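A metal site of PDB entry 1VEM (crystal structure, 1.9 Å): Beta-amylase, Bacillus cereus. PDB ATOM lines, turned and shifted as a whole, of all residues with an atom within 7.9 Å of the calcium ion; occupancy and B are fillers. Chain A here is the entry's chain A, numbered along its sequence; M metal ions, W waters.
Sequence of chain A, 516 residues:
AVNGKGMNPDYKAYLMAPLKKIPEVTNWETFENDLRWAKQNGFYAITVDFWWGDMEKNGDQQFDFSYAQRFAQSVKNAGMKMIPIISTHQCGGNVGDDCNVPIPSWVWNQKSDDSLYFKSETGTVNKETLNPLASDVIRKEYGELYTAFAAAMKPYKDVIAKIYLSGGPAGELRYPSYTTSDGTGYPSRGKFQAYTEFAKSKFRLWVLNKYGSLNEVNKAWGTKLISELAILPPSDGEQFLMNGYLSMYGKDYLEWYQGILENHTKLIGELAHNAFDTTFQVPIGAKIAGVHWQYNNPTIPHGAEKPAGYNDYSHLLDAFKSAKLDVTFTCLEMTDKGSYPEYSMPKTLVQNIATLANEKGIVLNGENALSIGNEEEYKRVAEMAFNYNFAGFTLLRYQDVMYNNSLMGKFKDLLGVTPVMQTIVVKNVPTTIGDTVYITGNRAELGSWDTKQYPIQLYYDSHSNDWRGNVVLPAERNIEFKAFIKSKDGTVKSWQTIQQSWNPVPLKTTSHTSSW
Water W1 lies within hydrogen-bond range of the backbone carbonyl oxygen (O) of Glu 141, the side-chain carboxylate (OE1) of Glu 56 and the backbone NH (N) of Leu 145.
The side-chain carboxylate (OD1) of Asp 60 binds the calcium ion (2.3 Å).
The calcium ion is bound by OE1 of Glu 144 (2.5 Å).
Water W1 is bound to the calcium ion (2.6 Å).
The side-chain carboxylate (OE1) of Glu 141 is bound to the calcium ion (2.6 Å).
The side-chain carboxylate (OE2) of Glu 56 is bound to the calcium ion, at 2.6 Å.
The calcium ion is bound by the side-chain amide oxygen (OE1) of Gln 61.
The calcium ion has six donor atoms within binding distance.
Within 4 Å of the calcium ion: Glu 56, Asp 60, Gln 61, Glu 141 and Glu 144.
The nearest printed residue that does not touch the calcium ion is Lys 140 (4.04 Å).
OE2 of Glu 144 lies within salt-bridge range of NZ of Lys 140.
OE1 of Glu 56 lies within hydrogen-bond range of NE1 of Trp 52 (2.8 Å).
OD2 of Asp 60 is in salt-bridge range of NZ of Lys 140 (3.2 Å).
OE2 of Glu 141 is in salt-bridge range of NZ of Lys 140 (2.9 Å).
OE1 of Gln 110 lies close to OE2 of Glu 141 (2.8 Å).
The indole nitrogen of Trp 106 lies within hydrogen-bond range of the backbone carbonyl oxygen of Glu 56 (2.8 Å).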
ATOM      1  N   TRP A  52     -24.836 -15.031  36.635  1.00  0.00           N
ATOM      2  CA  TRP A  52     -24.067 -15.034  35.399  1.00  0.00           C
ATOM      3  C   TRP A  52     -24.910 -14.306  34.358  1.00  0.00           C
ATOM      4  O   TRP A  52     -24.386 -13.560  33.532  1.00  0.00           O
ATOM      5  CB  TRP A  52     -23.801 -16.470  34.958  1.00  0.00           C
ATOM      6  CG  TRP A  52     -22.836 -16.611  33.807  1.00  0.00           C
ATOM      7  CD1 TRP A  52     -21.994 -15.643  33.326  1.00  0.00           C
ATOM      8  CD2 TRP A  52     -22.586 -17.787  33.034  1.00  0.00           C
ATOM      9  NE1 TRP A  52     -21.232 -16.159  32.294  1.00  0.00           N
ATOM     10  CE2 TRP A  52     -21.581 -17.472  32.097  1.00  0.00           C
ATOM     11  CE3 TRP A  52     -23.116 -19.090  33.054  1.00  0.00           C
ATOM     12  CZ2 TRP A  52     -21.087 -18.402  31.173  1.00  0.00           C
ATOM     13  CZ3 TRP A  52     -22.637 -20.018  32.128  1.00  0.00           C
ATOM     14  CH2 TRP A  52     -21.626 -19.673  31.206  1.00  0.00           C
ATOM     15  N   GLU A  56     -22.612 -11.278  32.399  1.00  0.00           N
ATOM     16  CA  GLU A  56     -22.084 -11.462  31.046  1.00  0.00           C
ATOM     17  C   GLU A  56     -23.267 -11.675  30.109  1.00  0.00           C
ATOM     18  O   GLU A  56     -23.274 -12.579  29.277  1.00  0.00           O
ATOM     19  CB  GLU A  56     -21.125 -12.664  31.039  1.00  0.00           C
ATOM     20  CG  GLU A  56     -20.283 -12.814  29.780  1.00  0.00           C
ATOM     21  CD  GLU A  56     -19.211 -13.903  29.906  1.00  0.00           C
ATOM     22  OE1 GLU A  56     -19.346 -14.793  30.783  1.00  0.00           O
ATOM     23  OE2 GLU A  56     -18.228 -13.875  29.126  1.00  0.00           O
ATOM     24  N   GLY A  59     -22.855 -10.592  25.772  1.00  0.00           N
ATOM     25  CA  GLY A  59     -22.075 -11.484  24.941  1.00  0.00           C
ATOM     26  C   GLY A  59     -20.797 -11.968  25.606  1.00  0.00           C
ATOM     27  O   GLY A  59     -20.460 -11.538  26.703  1.00  0.00           O
ATOM     28  N   ASP A  60     -20.094 -12.872  24.931  1.00  0.00           N
ATOM     29  CA  ASP A  60     -18.855 -13.423  25.456  1.00  0.00           C
ATOM     30  C   ASP A  60     -17.847 -12.305  25.758  1.00  0.00           C
ATOM     31  O   ASP A  60     -17.563 -11.463  24.912  1.00  0.00           O
ATOM     32  CB  ASP A  60     -18.272 -14.424  24.449  1.00  0.00           C
ATOM     33  CG  ASP A  60     -17.023 -15.109  24.970  1.00  0.00           C
ATOM     34  OD1 ASP A  60     -16.899 -15.288  26.200  1.00  0.00           O
ATOM     35  OD2 ASP A  60     -16.168 -15.496  24.149  1.00  0.00           O
ATOM     36  N   GLN A  61     -17.330 -12.315  26.989  1.00  0.00           N
ATOM     37  CA  GLN A  61     -16.346 -11.342  27.443  1.00  0.00           C
ATOM     38  C   GLN A  61     -16.868  -9.913  27.626  1.00  0.00           C
ATOM     39  O   GLN A  61     -16.081  -8.980  27.817  1.00  0.00           O
ATOM     40  CB  GLN A  61     -15.125 -11.332  26.517  1.00  0.00           C
ATOM     41  CG  GLN A  61     -14.330 -12.636  26.511  1.00  0.00           C
ATOM     42  CD  GLN A  61     -13.948 -13.104  27.907  1.00  0.00           C
ATOM     43  OE1 GLN A  61     -14.781 -13.630  28.646  1.00  0.00           O
ATOM     44  NE2 GLN A  61     -12.686 -12.910  28.279  1.00  0.00           N
ATOM     45  N   GLN A  62     -18.186  -9.734  27.548  1.00  0.00           N
ATOM     46  CA  GLN A  62     -18.797  -8.431  27.741  1.00  0.00           C
ATOM     47  C   GLN A  62     -19.342  -8.405  29.169  1.00  0.00           C
ATOM     48  O   GLN A  62     -20.534  -8.630  29.393  1.00  0.00           O
ATOM     49  CB  GLN A  62     -19.934  -8.216  26.745  1.00  0.00           C
ATOM     50  CG  GLN A  62     -19.483  -7.754  25.373  1.00  0.00           C
ATOM     51  CD  GLN A  62     -20.607  -7.776  24.355  1.00  0.00           C
ATOM     52  OE1 GLN A  62     -20.905  -8.822  23.777  1.00  0.00           O
ATOM     53  NE2 GLN A  62     -21.248  -6.629  24.162  1.00  0.00           N
ATOM     54  N   PHE A  63     -18.458  -8.135  30.121  1.00  0.00           N
ATOM     55  CA  PHE A  63     -18.798  -8.129  31.532  1.00  0.00           C
ATOM     56  C   PHE A  63     -19.353  -6.838  32.114  1.00  0.00           C
ATOM     57  O   PHE A  63     -19.100  -5.747  31.615  1.00  0.00           O
ATOM     58  CB  PHE A  63     -17.571  -8.528  32.357  1.00  0.00           C
ATOM     59  CG  PHE A  63     -17.034  -9.891  32.030  1.00  0.00           C
ATOM     60  CD1 PHE A  63     -17.769 -11.037  32.327  1.00  0.00           C
ATOM     61  CD2 PHE A  63     -15.797 -10.030  31.413  1.00  0.00           C
ATOM     62  CE1 PHE A  63     -17.271 -12.300  32.026  1.00  0.00           C
ATOM     63  CE2 PHE A  63     -15.285 -11.297  31.112  1.00  0.00           C
ATOM     64  CZ  PHE A  63     -16.028 -12.441  31.415  1.00  0.00           C
ATOM     65  N   TRP A 106     -26.398 -16.484  24.789  1.00  0.00           N
ATOM     66  CA  TRP A 106     -25.367 -16.756  23.790  1.00  0.00           C
ATOM     67  C   TRP A 106     -24.532 -18.010  24.074  1.00  0.00           C
ATOM     68  O   TRP A 106     -23.980 -18.595  23.148  1.00  0.00           O
ATOM     69  CB  TRP A 106     -24.422 -15.555  23.651  1.00  0.00           C
ATOM     70  CG  TRP A 106     -23.761 -15.143  24.922  1.00  0.00           C
ATOM     71  CD1 TRP A 106     -24.171 -14.159  25.776  1.00  0.00           C
ATOM     72  CD2 TRP A 106     -22.584 -15.712  25.503  1.00  0.00           C
ATOM     73  NE1 TRP A 106     -23.311 -14.084  26.860  1.00  0.00           N
ATOM     74  CE2 TRP A 106     -22.337 -15.028  26.713  1.00  0.00           C
ATOM     75  CE3 TRP A 106     -21.709 -16.744  25.116  1.00  0.00           C
ATOM     76  CZ2 TRP A 106     -21.252 -15.339  27.548  1.00  0.00           C
ATOM     77  CZ3 TRP A 106     -20.630 -17.053  25.944  1.00  0.00           C
ATOM     78  CH2 TRP A 106     -20.415 -16.344  27.146  1.00  0.00           C
ATOM     79  N   GLN A 110     -22.494 -22.016  21.422  1.00  0.00           N
ATOM     80  CA  GLN A 110     -21.103 -22.439  21.281  1.00  0.00           C
ATOM     81  C   GLN A 110     -20.950 -23.893  20.874  1.00  0.00           C
ATOM     82  O   GLN A 110     -19.831 -24.387  20.703  1.00  0.00           O
ATOM     83  CB  GLN A 110     -20.330 -22.190  22.585  1.00  0.00           C
ATOM     84  CG  GLN A 110     -19.941 -20.742  22.780  1.00  0.00           C
ATOM     85  CD  GLN A 110     -18.817 -20.568  23.794  1.00  0.00           C
ATOM     86  OE1 GLN A 110     -18.272 -19.477  23.949  1.00  0.00           O
ATOM     87  NE2 GLN A 110     -18.468 -21.657  24.484  1.00  0.00           N
ATOM     88  N   VAL A 137     -16.191 -26.411  27.563  1.00  0.00           N
ATOM     89  CA  VAL A 137     -16.906 -25.143  27.599  1.00  0.00           C
ATOM     90  C   VAL A 137     -16.880 -24.575  29.014  1.00  0.00           C
ATOM     91  O   VAL A 137     -16.669 -23.379  29.212  1.00  0.00           O
ATOM     92  CB  VAL A 137     -18.378 -25.309  27.154  1.00  0.00           C
ATOM     93  CG1 VAL A 137     -19.165 -24.052  27.451  1.00  0.00           C
ATOM     94  CG2 VAL A 137     -18.431 -25.609  25.654  1.00  0.00           C
ATOM     95  N   LYS A 140     -13.508 -22.982  29.836  1.00  0.00           N
ATOM     96  CA  LYS A 140     -13.348 -21.672  29.238  1.00  0.00           C
ATOM     97  C   LYS A 140     -14.221 -20.603  29.893  1.00  0.00           C
ATOM     98  O   LYS A 140     -13.716 -19.609  30.405  1.00  0.00           O
ATOM     99  CB  LYS A 140     -13.671 -21.726  27.743  1.00  0.00           C
ATOM    100  CG  LYS A 140     -13.641 -20.353  27.057  1.00  0.00           C
ATOM    101  CD  LYS A 140     -14.006 -20.439  25.584  1.00  0.00           C
ATOM    102  CE  LYS A 140     -14.031 -19.044  24.939  1.00  0.00           C
ATOM    103  NZ  LYS A 140     -15.119 -18.171  25.490  1.00  0.00           N
ATOM    104  N   GLU A 141     -15.541 -20.809  29.868  1.00  0.00           N
ATOM    105  CA  GLU A 141     -16.482 -19.842  30.418  1.00  0.00           C
ATOM    106  C   GLU A 141     -16.338 -19.519  31.905  1.00  0.00           C
ATOM    107  O   GLU A 141     -16.310 -18.355  32.285  1.00  0.00           O
ATOM    108  CB  GLU A 141     -17.923 -20.286  30.136  1.00  0.00           C
ATOM    109  CG  GLU A 141     -18.272 -20.436  28.664  1.00  0.00           C
ATOM    110  CD  GLU A 141     -17.771 -19.290  27.799  1.00  0.00           C
ATOM    111  OE1 GLU A 141     -17.766 -18.129  28.271  1.00  0.00           O
ATOM    112  OE2 GLU A 141     -17.383 -19.554  26.636  1.00  0.00           O
ATOM    113  N   TYR A 142     -16.263 -20.553  32.753  1.00  0.00           N
ATOM    114  CA  TYR A 142     -16.133 -20.310  34.198  1.00  0.00           C
ATOM    115  C   TYR A 142     -14.764 -19.710  34.476  1.00  0.00           C
ATOM    116  O   TYR A 142     -14.632 -18.830  35.325  1.00  0.00           O
ATOM    117  CB  TYR A 142     -16.289 -21.616  34.987  1.00  0.00           C
ATOM    118  CG  TYR A 142     -17.700 -22.168  35.089  1.00  0.00           C
ATOM    119  CD1 TYR A 142     -18.631 -21.973  34.075  1.00  0.00           C
ATOM    120  CD2 TYR A 142     -18.078 -22.956  36.187  1.00  0.00           C
ATOM    121  CE1 TYR A 142     -19.916 -22.550  34.138  1.00  0.00           C
ATOM    122  CE2 TYR A 142     -19.343 -23.537  36.257  1.00  0.00           C
ATOM    123  CZ  TYR A 142     -20.258 -23.335  35.229  1.00  0.00           C
ATOM    124  OH  TYR A 142     -21.498 -23.942  35.271  1.00  0.00           O
ATOM    125  N   GLY A 143     -13.757 -20.195  33.758  1.00  0.00           N
ATOM    126  CA  GLY A 143     -12.411 -19.695  33.946  1.00  0.00           C
ATOM    127  C   GLY A 143     -12.359 -18.203  33.689  1.00  0.00           C
ATOM    128  O   GLY A 143     -11.785 -17.460  34.484  1.00  0.00           O
ATOM    129  N   GLU A 144     -12.962 -17.767  32.595  1.00  0.00           N
ATOM    130  CA  GLU A 144     -12.973 -16.347  32.247  1.00  0.00           C
ATOM    131  C   GLU A 144     -13.829 -15.539  33.220  1.00  0.00           C
ATOM    132  O   GLU A 144     -13.433 -14.444  33.643  1.00  0.00           O
ATOM    133  CB  GLU A 144     -13.481 -16.161  30.814  1.00  0.00           C
ATOM    134  CG  GLU A 144     -12.590 -16.865  29.782  1.00  0.00           C
ATOM    135  CD  GLU A 144     -13.079 -16.692  28.357  1.00  0.00           C
ATOM    136  OE1 GLU A 144     -14.303 -16.789  28.132  1.00  0.00           O
ATOM    137  OE2 GLU A 144     -12.237 -16.477  27.464  1.00  0.00           O
ATOM    138  N   LEU A 145     -14.984 -16.083  33.595  1.00  0.00           N
ATOM    139  CA  LEU A 145     -15.878 -15.401  34.528  1.00  0.00           C
ATOM    140  C   LEU A 145     -15.201 -15.204  35.890  1.00  0.00           C
ATOM    141  O   LEU A 145     -15.194 -14.103  36.434  1.00  0.00           O
ATOM    142  CB  LEU A 145     -17.176 -16.187  34.709  1.00  0.00           C
ATOM    143  CG  LEU A 145     -18.198 -15.572  35.670  1.00  0.00           C
ATOM    144  CD1 LEU A 145     -18.571 -14.177  35.220  1.00  0.00           C
ATOM    145  CD2 LEU A 145     -19.435 -16.464  35.734  1.00  0.00           C
HETATM  146 CA    CA M   1     -16.569 -15.808  28.432  1.00  0.00          CA
HETATM  147  O   HOH W   1     -16.991 -16.168  30.933  1.00  0.00           O
